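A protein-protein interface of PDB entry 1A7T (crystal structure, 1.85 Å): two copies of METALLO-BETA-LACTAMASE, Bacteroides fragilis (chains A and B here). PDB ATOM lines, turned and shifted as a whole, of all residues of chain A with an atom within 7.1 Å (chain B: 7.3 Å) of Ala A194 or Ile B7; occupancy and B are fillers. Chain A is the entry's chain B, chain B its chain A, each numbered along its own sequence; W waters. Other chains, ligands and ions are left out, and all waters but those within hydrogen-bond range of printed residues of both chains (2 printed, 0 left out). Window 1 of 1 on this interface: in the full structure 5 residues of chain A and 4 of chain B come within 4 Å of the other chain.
Printed residues of chain B within 4 Å of Lys A191: Met B62 (3.7 Å).
Of chain A, only Ala A194 comes within 4 Å of Ile B7.
Of the printed residues of chain A, Met B62 touches Lys A191 (3.7 Å).
Val B64 touches none of the printed residues of chain A.
Asn B65 touches none of the printed residues of chain A.
The nearest printed residue of chain A that does not touch Asp B69 is Ala A194 (5.6 Å).
Of the 21 printed residues of chain B, 4 touch a printed residue of chain A.
Hydrophobic or aromatic side chains of chain B that line the printed part of chain A: Met B62.
Among the printed residues, Asp or Glu carboxylates within 4 Å of a Lys or Arg side-chain nitrogen of the other chain: Lys A195 with Asp B69 (3.98 Å).
The side-chain carboxylate of Asp B69 lies within salt-bridge range of the side-chain amino group of Lys A195 (3.98 Å).
The side-chain hydroxyl (OG) of Ser B8 lies close to the side-chain sulfur (SD) of Met B62 (3.6 Å).
No position is printed for both chains.
Of the 4 pairs that touch across the chains among the printed residues, none has its exchanged pair printed and touching as well.
Asp A190 touches Asp B9.
CE of Met B62 touches CG of Lys A191, 3.7 Å away.
CB of Ala A194 touches O of Ile B7, 3.7 Å away.
Water W1 lies within hydrogen-bond range of NZ of Lys A195 and ND2 of Asn B65.
Water W2 lies within hydrogen-bond range of OD2 of Asp A190 and OD2 of Asp B10.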
ATOM      1  N   THR A 188       3.211 -13.071 -33.901  1.00  0.00           N
ATOM      2  CA  THR A 188       2.147 -12.990 -34.918  1.00  0.00           C
ATOM      3  C   THR A 188       1.722 -14.420 -35.256  1.00  0.00           C
ATOM      4  O   THR A 188       0.546 -14.781 -35.428  1.00  0.00           O
ATOM      5  CB  THR A 188       2.747 -12.311 -36.168  1.00  0.00           C
ATOM      6  OG1 THR A 188       3.067 -10.974 -35.796  1.00  0.00           O
ATOM      7  CG2 THR A 188       1.720 -12.344 -37.326  1.00  0.00           C
ATOM      8  N   LEU A 189       2.735 -15.285 -35.317  1.00  0.00           N
ATOM      9  CA  LEU A 189       2.517 -16.710 -35.624  1.00  0.00           C
ATOM     10  C   LEU A 189       1.719 -17.391 -34.531  1.00  0.00           C
ATOM     11  O   LEU A 189       0.826 -18.221 -34.858  1.00  0.00           O
ATOM     12  CB  LEU A 189       3.832 -17.457 -35.897  1.00  0.00           C
ATOM     13  CG  LEU A 189       4.514 -17.009 -37.215  1.00  0.00           C
ATOM     14  CD1 LEU A 189       5.896 -17.624 -37.333  1.00  0.00           C
ATOM     15  CD2 LEU A 189       3.629 -17.327 -38.416  1.00  0.00           C
ATOM     16  N   ASP A 190       2.008 -17.081 -33.277  1.00  0.00           N
ATOM     17  CA  ASP A 190       1.231 -17.675 -32.172  1.00  0.00           C
ATOM     18  C   ASP A 190      -0.240 -17.218 -32.235  1.00  0.00           C
ATOM     19  O   ASP A 190      -1.161 -18.013 -31.922  1.00  0.00           O
ATOM     20  CB  ASP A 190       1.780 -17.122 -30.855  1.00  0.00           C
ATOM     21  CG  ASP A 190       2.993 -17.866 -30.371  1.00  0.00           C
ATOM     22  OD1 ASP A 190       3.136 -19.001 -30.870  1.00  0.00           O
ATOM     23  OD2 ASP A 190       3.818 -17.317 -29.548  1.00  0.00           O
ATOM     24  N   LYS A 191      -0.469 -15.974 -32.613  1.00  0.00           N
ATOM     25  CA  LYS A 191      -1.798 -15.401 -32.742  1.00  0.00           C
ATOM     26  C   LYS A 191      -2.552 -16.087 -33.898  1.00  0.00           C
ATOM     27  O   LYS A 191      -3.686 -16.487 -33.713  1.00  0.00           O
ATOM     28  CB  LYS A 191      -1.777 -13.898 -33.068  1.00  0.00           C
ATOM     29  CG  LYS A 191      -1.327 -13.089 -31.865  1.00  0.00           C
ATOM     30  CD  LYS A 191      -1.370 -11.615 -32.167  1.00  0.00           C
ATOM     31  CE  LYS A 191      -0.247 -10.955 -31.384  1.00  0.00           C
ATOM     32  NZ  LYS A 191       0.472  -9.974 -32.293  1.00  0.00           N
ATOM     33  N   VAL A 192      -1.891 -16.264 -35.035  1.00  0.00           N
ATOM     34  CA  VAL A 192      -2.532 -16.970 -36.144  1.00  0.00           C
ATOM     35  C   VAL A 192      -2.955 -18.381 -35.736  1.00  0.00           C
ATOM     36  O   VAL A 192      -4.072 -18.815 -35.991  1.00  0.00           O
ATOM     37  CB  VAL A 192      -1.518 -17.039 -37.299  1.00  0.00           C
ATOM     38  CG1 VAL A 192      -2.059 -17.938 -38.391  1.00  0.00           C
ATOM     39  CG2 VAL A 192      -1.272 -15.609 -37.825  1.00  0.00           C
ATOM     40  N   LYS A 193      -2.065 -19.104 -35.097  1.00  0.00           N
ATOM     41  CA  LYS A 193      -2.278 -20.438 -34.603  1.00  0.00           C
ATOM     42  C   LYS A 193      -3.447 -20.531 -33.609  1.00  0.00           C
ATOM     43  O   LYS A 193      -4.294 -21.441 -33.729  1.00  0.00           O
ATOM     44  CB  LYS A 193      -1.028 -20.923 -33.827  1.00  0.00           C
ATOM     45  CG  LYS A 193      -1.228 -22.361 -33.398  1.00  0.00           C
ATOM     46  CD  LYS A 193       0.086 -23.026 -32.974  1.00  0.00           C
ATOM     47  CE  LYS A 193      -0.234 -24.528 -32.779  1.00  0.00           C
ATOM     48  NZ  LYS A 193      -1.007 -25.096 -33.963  1.00  0.00           N
ATOM     49  N   ALA A 194      -3.470 -19.583 -32.666  1.00  0.00           N
ATOM     50  CA  ALA A 194      -4.538 -19.550 -31.678  1.00  0.00           C
ATOM     51  C   ALA A 194      -5.871 -19.208 -32.268  1.00  0.00           C
ATOM     52  O   ALA A 194      -6.936 -19.730 -31.873  1.00  0.00           O
ATOM     53  CB  ALA A 194      -4.208 -18.515 -30.579  1.00  0.00           C
ATOM     54  N   LYS A 195      -5.925 -18.364 -33.289  1.00  0.00           N
ATOM     55  CA  LYS A 195      -7.204 -17.965 -33.896  1.00  0.00           C
ATOM     56  C   LYS A 195      -7.787 -18.964 -34.856  1.00  0.00           C
ATOM     57  O   LYS A 195      -9.004 -18.903 -35.062  1.00  0.00           O
ATOM     58  CB  LYS A 195      -6.909 -16.673 -34.689  1.00  0.00           C
ATOM     59  CG  LYS A 195      -8.038 -15.717 -34.979  1.00  0.00           C
ATOM     60  CD  LYS A 195      -7.467 -14.287 -34.925  1.00  0.00           C
ATOM     61  CE  LYS A 195      -8.621 -13.367 -35.413  1.00  0.00           C
ATOM     62  NZ  LYS A 195      -9.812 -13.658 -34.553  1.00  0.00           N
ATOM     63  N   PHE A 196      -7.012 -19.803 -35.523  1.00  0.00           N
ATOM     64  CA  PHE A 196      -7.628 -20.672 -36.541  1.00  0.00           C
ATOM     65  C   PHE A 196      -7.294 -22.105 -36.315  1.00  0.00           C
ATOM     66  O   PHE A 196      -6.610 -22.784 -37.077  1.00  0.00           O
ATOM     67  CB  PHE A 196      -7.125 -20.226 -37.942  1.00  0.00           C
ATOM     68  CG  PHE A 196      -7.313 -18.761 -38.190  1.00  0.00           C
ATOM     69  CD1 PHE A 196      -8.566 -18.212 -38.452  1.00  0.00           C
ATOM     70  CD2 PHE A 196      -6.196 -17.910 -38.204  1.00  0.00           C
ATOM     71  CE1 PHE A 196      -8.713 -16.837 -38.686  1.00  0.00           C
ATOM     72  CE2 PHE A 196      -6.343 -16.543 -38.422  1.00  0.00           C
ATOM     73  CZ  PHE A 196      -7.583 -16.000 -38.651  1.00  0.00           C
ATOM     74  N   PRO A 197      -7.732 -22.612 -35.152  1.00  0.00           N
ATOM     75  CA  PRO A 197      -7.478 -24.016 -34.820  1.00  0.00           C
ATOM     76  C   PRO A 197      -8.206 -24.991 -35.742  1.00  0.00           C
ATOM     77  O   PRO A 197      -7.784 -26.166 -35.810  1.00  0.00           O
ATOM     78  CB  PRO A 197      -7.926 -24.084 -33.361  1.00  0.00           C
ATOM     79  CG  PRO A 197      -9.056 -23.072 -33.311  1.00  0.00           C
ATOM     80  CD  PRO A 197      -8.544 -21.897 -34.137  1.00  0.00           C
ATOM     81  N   ILE A 215       2.700 -23.488 -39.612  1.00  0.00           N
ATOM     82  CA  ILE A 215       2.811 -22.456 -38.608  1.00  0.00           C
ATOM     83  C   ILE A 215       3.885 -22.806 -37.595  1.00  0.00           C
ATOM     84  O   ILE A 215       4.744 -21.923 -37.299  1.00  0.00           O
ATOM     85  CB  ILE A 215       1.461 -22.243 -37.870  1.00  0.00           C
ATOM     86  CG1 ILE A 215       0.400 -21.746 -38.866  1.00  0.00           C
ATOM     87  CG2 ILE A 215       1.651 -21.133 -36.815  1.00  0.00           C
ATOM     88  CD1 ILE A 215      -1.032 -22.062 -38.363  1.00  0.00           C
ATOM     89  N   SER B   4      -5.247 -30.627 -20.137  1.00  0.00           N
ATOM     90  CA  SER B   4      -4.983 -29.260 -20.519  1.00  0.00           C
ATOM     91  C   SER B   4      -5.155 -29.052 -22.011  1.00  0.00           C
ATOM     92  O   SER B   4      -5.211 -29.962 -22.821  1.00  0.00           O
ATOM     93  CB  SER B   4      -3.532 -28.877 -20.208  1.00  0.00           C
ATOM     94  OG  SER B   4      -3.197 -29.255 -18.882  1.00  0.00           O
ATOM     95  N   VAL B   5      -5.250 -27.815 -22.411  1.00  0.00           N
ATOM     96  CA  VAL B   5      -5.365 -27.400 -23.811  1.00  0.00           C
ATOM     97  C   VAL B   5      -4.381 -26.226 -23.943  1.00  0.00           C
ATOM     98  O   VAL B   5      -4.542 -25.220 -23.257  1.00  0.00           O
ATOM     99  CB  VAL B   5      -6.792 -26.911 -24.113  1.00  0.00           C
ATOM    100  CG1 VAL B   5      -6.891 -26.293 -25.492  1.00  0.00           C
ATOM    101  CG2 VAL B   5      -7.796 -28.055 -23.991  1.00  0.00           C
ATOM    102  N   LYS B   6      -3.349 -26.389 -24.753  1.00  0.00           N
ATOM    103  CA  LYS B   6      -2.369 -25.333 -24.949  1.00  0.00           C
ATOM    104  C   LYS B   6      -2.908 -24.314 -25.936  1.00  0.00           C
ATOM    105  O   LYS B   6      -2.839 -24.563 -27.142  1.00  0.00           O
ATOM    106  CB  LYS B   6      -1.066 -25.881 -25.511  1.00  0.00           C
ATOM    107  CG  LYS B   6      -0.040 -26.258 -24.442  1.00  0.00           C
ATOM    108  CD  LYS B   6       0.442 -27.690 -24.586  1.00  0.00           C
ATOM    109  CE  LYS B   6      -0.128 -28.692 -23.583  1.00  0.00           C
ATOM    110  NZ  LYS B   6       0.853 -29.064 -22.493  1.00  0.00           N
ATOM    111  N   ILE B   7      -3.433 -23.209 -25.470  1.00  0.00           N
ATOM    112  CA  ILE B   7      -3.958 -22.221 -26.426  1.00  0.00           C
ATOM    113  C   ILE B   7      -2.811 -21.526 -27.135  1.00  0.00           C
ATOM    114  O   ILE B   7      -2.941 -21.098 -28.277  1.00  0.00           O
ATOM    115  CB  ILE B   7      -5.007 -21.323 -25.821  1.00  0.00           C
ATOM    116  CG1 ILE B   7      -4.454 -20.176 -24.980  1.00  0.00           C
ATOM    117  CG2 ILE B   7      -5.908 -22.172 -24.906  1.00  0.00           C
ATOM    118  CD1 ILE B   7      -5.570 -19.496 -24.192  1.00  0.00           C
ATOM    119  N   SER B   8      -1.636 -21.433 -26.489  1.00  0.00           N
ATOM    120  CA  SER B   8      -0.485 -20.846 -27.150  1.00  0.00           C
ATOM    121  C   SER B   8       0.805 -21.396 -26.560  1.00  0.00           C
ATOM    122  O   SER B   8       0.836 -22.347 -25.805  1.00  0.00           O
ATOM    123  CB  SER B   8      -0.375 -19.339 -27.097  1.00  0.00           C
ATOM    124  OG  SER B   8      -0.128 -18.867 -25.792  1.00  0.00           O
ATOM    125  N   ASP B   9       1.879 -20.690 -26.943  1.00  0.00           N
ATOM    126  CA  ASP B   9       3.201 -21.102 -26.477  1.00  0.00           C
ATOM    127  C   ASP B   9       3.346 -20.907 -24.988  1.00  0.00           C
ATOM    128  O   ASP B   9       3.890 -21.798 -24.319  1.00  0.00           O
ATOM    129  CB  ASP B   9       4.296 -20.433 -27.326  1.00  0.00           C
ATOM    130  CG  ASP B   9       4.885 -21.488 -28.280  1.00  0.00           C
ATOM    131  OD1 ASP B   9       4.151 -22.113 -29.088  1.00  0.00           O
ATOM    132  OD2 ASP B   9       6.109 -21.766 -28.176  1.00  0.00           O
ATOM    133  N   ASP B  10       2.801 -19.855 -24.400  1.00  0.00           N
ATOM    134  CA  ASP B  10       2.886 -19.595 -22.980  1.00  0.00           C
ATOM    135  C   ASP B  10       1.605 -19.798 -22.166  1.00  0.00           C
ATOM    136  O   ASP B  10       1.578 -19.385 -20.997  1.00  0.00           O
ATOM    137  CB  ASP B  10       3.083 -18.079 -22.792  1.00  0.00           C
ATOM    138  CG  ASP B  10       3.542 -17.155 -23.837  1.00  0.00           C
ATOM    139  OD1 ASP B  10       4.764 -17.248 -24.188  1.00  0.00           O
ATOM    140  OD2 ASP B  10       2.796 -16.232 -24.288  1.00  0.00           O
ATOM    141  N   ILE B  11       0.522 -20.258 -22.794  1.00  0.00           N
ATOM    142  CA  ILE B  11      -0.732 -20.348 -22.001  1.00  0.00           C
ATOM    143  C   ILE B  11      -1.431 -21.663 -22.246  1.00  0.00           C
ATOM    144  O   ILE B  11      -1.580 -22.101 -23.403  1.00  0.00           O
ATOM    145  CB  ILE B  11      -1.670 -19.211 -22.424  1.00  0.00           C
ATOM    146  CG1 ILE B  11      -0.993 -17.847 -22.168  1.00  0.00           C
ATOM    147  CG2 ILE B  11      -2.962 -19.173 -21.604  1.00  0.00           C
ATOM    148  CD1 ILE B  11      -1.897 -16.706 -22.644  1.00  0.00           C
ATOM    149  N   SER B  12      -1.826 -22.293 -21.141  1.00  0.00           N
ATOM    150  CA  SER B  12      -2.568 -23.560 -21.280  1.00  0.00           C
ATOM    151  C   SER B  12      -3.762 -23.411 -20.341  1.00  0.00           C
ATOM    152  O   SER B  12      -3.727 -22.544 -19.437  1.00  0.00           O
ATOM    153  CB  SER B  12      -1.679 -24.740 -21.028  1.00  0.00           C
ATOM    154  OG  SER B  12      -1.277 -24.714 -19.654  1.00  0.00           O
ATOM    155  N   ILE B  13      -4.803 -24.163 -20.584  1.00  0.00           N
ATOM    156  CA  ILE B  13      -6.044 -24.095 -19.845  1.00  0.00           C
ATOM    157  C   ILE B  13      -6.521 -25.477 -19.445  1.00  0.00           C
ATOM    158  O   ILE B  13      -6.385 -26.408 -20.283  1.00  0.00           O
ATOM    159  CB  ILE B  13      -7.180 -23.628 -20.813  1.00  0.00           C
ATOM    160  CG1 ILE B  13      -6.711 -22.404 -21.575  1.00  0.00           C
ATOM    161  CG2 ILE B  13      -8.401 -23.253 -20.002  1.00  0.00           C
ATOM    162  CD1 ILE B  13      -6.465 -21.283 -20.573  1.00  0.00           C
ATOM    163  N   TYR B  23      -6.263 -21.451 -15.810  1.00  0.00           N
ATOM    164  CA  TYR B  23      -5.222 -21.279 -16.788  1.00  0.00           C
ATOM    165  C   TYR B  23      -3.844 -21.121 -16.112  1.00  0.00           C
ATOM    166  O   TYR B  23      -3.745 -20.679 -14.986  1.00  0.00           O
ATOM    167  CB  TYR B  23      -5.400 -20.044 -17.735  1.00  0.00           C
ATOM    168  CG  TYR B  23      -5.270 -18.712 -17.067  1.00  0.00           C
ATOM    169  CD1 TYR B  23      -6.387 -18.069 -16.499  1.00  0.00           C
ATOM    170  CD2 TYR B  23      -4.005 -18.073 -16.972  1.00  0.00           C
ATOM    171  CE1 TYR B  23      -6.280 -16.834 -15.882  1.00  0.00           C
ATOM    172  CE2 TYR B  23      -3.892 -16.862 -16.291  1.00  0.00           C
ATOM    173  CZ  TYR B  23      -5.046 -16.244 -15.803  1.00  0.00           C
ATOM    174  OH  TYR B  23      -4.891 -15.059 -15.135  1.00  0.00           O
ATOM    175  N   ILE B  41     -11.045 -18.831 -15.001  1.00  0.00           N
ATOM    176  CA  ILE B  41     -12.021 -18.354 -15.975  1.00  0.00           C
ATOM    177  C   ILE B  41     -13.346 -18.978 -15.549  1.00  0.00           C
ATOM    178  O   ILE B  41     -13.400 -20.218 -15.374  1.00  0.00           O
ATOM    179  CB  ILE B  41     -11.651 -18.729 -17.404  1.00  0.00           C
ATOM    180  CG1 ILE B  41     -10.324 -18.126 -17.870  1.00  0.00           C
ATOM    181  CG2 ILE B  41     -12.739 -18.088 -18.308  1.00  0.00           C
ATOM    182  CD1 ILE B  41      -9.724 -18.839 -19.059  1.00  0.00           C
ATOM    183  N   GLN B  59      -0.520 -11.076 -23.185  1.00  0.00           N
ATOM    184  CA  GLN B  59      -0.986 -12.404 -22.817  1.00  0.00           C
ATOM    185  C   GLN B  59      -2.441 -12.328 -22.372  1.00  0.00           C
ATOM    186  O   GLN B  59      -3.243 -13.266 -22.639  1.00  0.00           O
ATOM    187  CB  GLN B  59      -0.118 -12.934 -21.686  1.00  0.00           C
ATOM    188  CG  GLN B  59       1.325 -13.263 -22.165  1.00  0.00           C
ATOM    189  CD  GLN B  59       1.989 -14.170 -21.162  1.00  0.00           C
ATOM    190  OE1 GLN B  59       1.739 -14.080 -19.928  1.00  0.00           O
ATOM    191  NE2 GLN B  59       2.892 -15.040 -21.517  1.00  0.00           N
ATOM    192  N   MET B  62      -4.566 -12.211 -25.436  1.00  0.00           N
ATOM    193  CA  MET B  62      -4.654 -13.522 -26.107  1.00  0.00           C
ATOM    194  C   MET B  62      -5.628 -14.446 -25.388  1.00  0.00           C
ATOM    195  O   MET B  62      -6.390 -15.255 -25.952  1.00  0.00           O
ATOM    196  CB  MET B  62      -3.262 -14.120 -26.245  1.00  0.00           C
ATOM    197  CG  MET B  62      -3.155 -15.613 -26.437  1.00  0.00           C
ATOM    198  SD  MET B  62      -1.800 -16.165 -27.484  1.00  0.00           S
ATOM    199  CE  MET B  62      -2.033 -15.104 -28.897  1.00  0.00           C
ATOM    200  N   LEU B  63      -5.622 -14.374 -24.069  1.00  0.00           N
ATOM    201  CA  LEU B  63      -6.504 -15.222 -23.226  1.00  0.00           C
ATOM    202  C   LEU B  63      -7.954 -14.810 -23.388  1.00  0.00           C
ATOM    203  O   LEU B  63      -8.896 -15.669 -23.506  1.00  0.00           O
ATOM    204  CB  LEU B  63      -6.089 -15.002 -21.746  1.00  0.00           C
ATOM    205  CG  LEU B  63      -6.899 -15.821 -20.716  1.00  0.00           C
ATOM    206  CD1 LEU B  63      -6.813 -17.299 -20.997  1.00  0.00           C
ATOM    207  CD2 LEU B  63      -6.396 -15.576 -19.305  1.00  0.00           C
ATOM    208  N   VAL B  64      -8.215 -13.528 -23.408  1.00  0.00           N
ATOM    209  CA  VAL B  64      -9.584 -13.013 -23.557  1.00  0.00           C
ATOM    210  C   VAL B  64     -10.127 -13.372 -24.947  1.00  0.00           C
ATOM    211  O   VAL B  64     -11.301 -13.729 -25.086  1.00  0.00           O
ATOM    212  CB  VAL B  64      -9.642 -11.522 -23.292  1.00  0.00           C
ATOM    213  CG1 VAL B  64     -11.005 -10.923 -23.633  1.00  0.00           C
ATOM    214  CG2 VAL B  64      -9.440 -11.216 -21.799  1.00  0.00           C
ATOM    215  N   ASN B  65      -9.271 -13.308 -25.978  1.00  0.00           N
ATOM    216  CA  ASN B  65      -9.689 -13.636 -27.352  1.00  0.00           C
ATOM    217  C   ASN B  65     -10.077 -15.094 -27.404  1.00  0.00           C
ATOM    218  O   ASN B  65     -10.986 -15.478 -28.125  1.00  0.00           O
ATOM    219  CB  ASN B  65      -8.561 -13.365 -28.352  1.00  0.00           C
ATOM    220  CG  ASN B  65      -8.400 -11.923 -28.739  1.00  0.00           C
ATOM    221  OD1 ASN B  65      -9.186 -11.036 -28.408  1.00  0.00           O
ATOM    222  ND2 ASN B  65      -7.406 -11.505 -29.547  1.00  0.00           N
ATOM    223  N   TRP B  66      -9.425 -15.976 -26.653  1.00  0.00           N
ATOM    224  CA  TRP B  66      -9.708 -17.399 -26.651  1.00  0.00           C
ATOM    225  C   TRP B  66     -11.020 -17.698 -25.964  1.00  0.00           C
ATOM    226  O   TRP B  66     -11.801 -18.572 -26.369  1.00  0.00           O
ATOM    227  CB  TRP B  66      -8.557 -18.229 -26.064  1.00  0.00           C
ATOM    228  CG  TRP B  66      -8.809 -19.706 -26.003  1.00  0.00           C
ATOM    229  CD1 TRP B  66      -8.526 -20.648 -26.958  1.00  0.00           C
ATOM    230  CD2 TRP B  66      -9.443 -20.432 -24.933  1.00  0.00           C
ATOM    231  NE1 TRP B  66      -8.956 -21.909 -26.547  1.00  0.00           N
ATOM    232  CE2 TRP B  66      -9.507 -21.788 -25.302  1.00  0.00           C
ATOM    233  CE3 TRP B  66      -9.953 -20.042 -23.689  1.00  0.00           C
ATOM    234  CZ2 TRP B  66     -10.060 -22.759 -24.493  1.00  0.00           C
ATOM    235  CZ3 TRP B  66     -10.481 -21.000 -22.847  1.00  0.00           C
ATOM    236  CH2 TRP B  66     -10.549 -22.345 -23.263  1.00  0.00           C
ATOM    237  N   VAL B  67     -11.326 -16.957 -24.906  1.00  0.00           N
ATOM    238  CA  VAL B  67     -12.566 -17.210 -24.161  1.00  0.00           C
ATOM    239  C   VAL B  67     -13.719 -16.877 -25.093  1.00  0.00           C
ATOM    240  O   VAL B  67     -14.686 -17.612 -25.195  1.00  0.00           O
ATOM    241  CB  VAL B  67     -12.655 -16.341 -22.893  1.00  0.00           C
ATOM    242  CG1 VAL B  67     -14.004 -16.432 -22.222  1.00  0.00           C
ATOM    243  CG2 VAL B  67     -11.541 -16.783 -21.918  1.00  0.00           C
ATOM    244  N   ASP B  69     -13.751 -16.607 -28.645  1.00  0.00           N
ATOM    245  CA  ASP B  69     -13.761 -17.518 -29.757  1.00  0.00           C
ATOM    246  C   ASP B  69     -13.938 -18.989 -29.419  1.00  0.00           C
ATOM    247  O   ASP B  69     -14.621 -19.703 -30.172  1.00  0.00           O
ATOM    248  CB  ASP B  69     -12.427 -17.513 -30.521  1.00  0.00           C
ATOM    249  CG  ASP B  69     -12.128 -16.189 -31.140  1.00  0.00           C
ATOM    250  OD1 ASP B  69     -13.091 -15.401 -31.219  1.00  0.00           O
ATOM    251  OD2 ASP B  69     -10.966 -15.872 -31.459  1.00  0.00           O
ATOM    252  N   SER B  70     -13.359 -19.538 -28.375  1.00  0.00           N
ATOM    253  CA  SER B  70     -13.479 -20.929 -28.091  1.00  0.00           C
ATOM    254  C   SER B  70     -14.445 -21.232 -26.992  1.00  0.00           C
ATOM    255  O   SER B  70     -15.026 -22.328 -27.054  1.00  0.00           O
ATOM    256  CB  SER B  70     -12.136 -21.596 -27.854  1.00  0.00           C
ATOM    257  OG  SER B  70     -11.317 -21.429 -29.006  1.00  0.00           O
HETATM  258  O   HOH W   1      -8.477 -12.735 -32.563  1.00  0.00           O
HETATM  259  O   HOH W   2       2.322 -16.186 -27.291  1.00  0.00           O
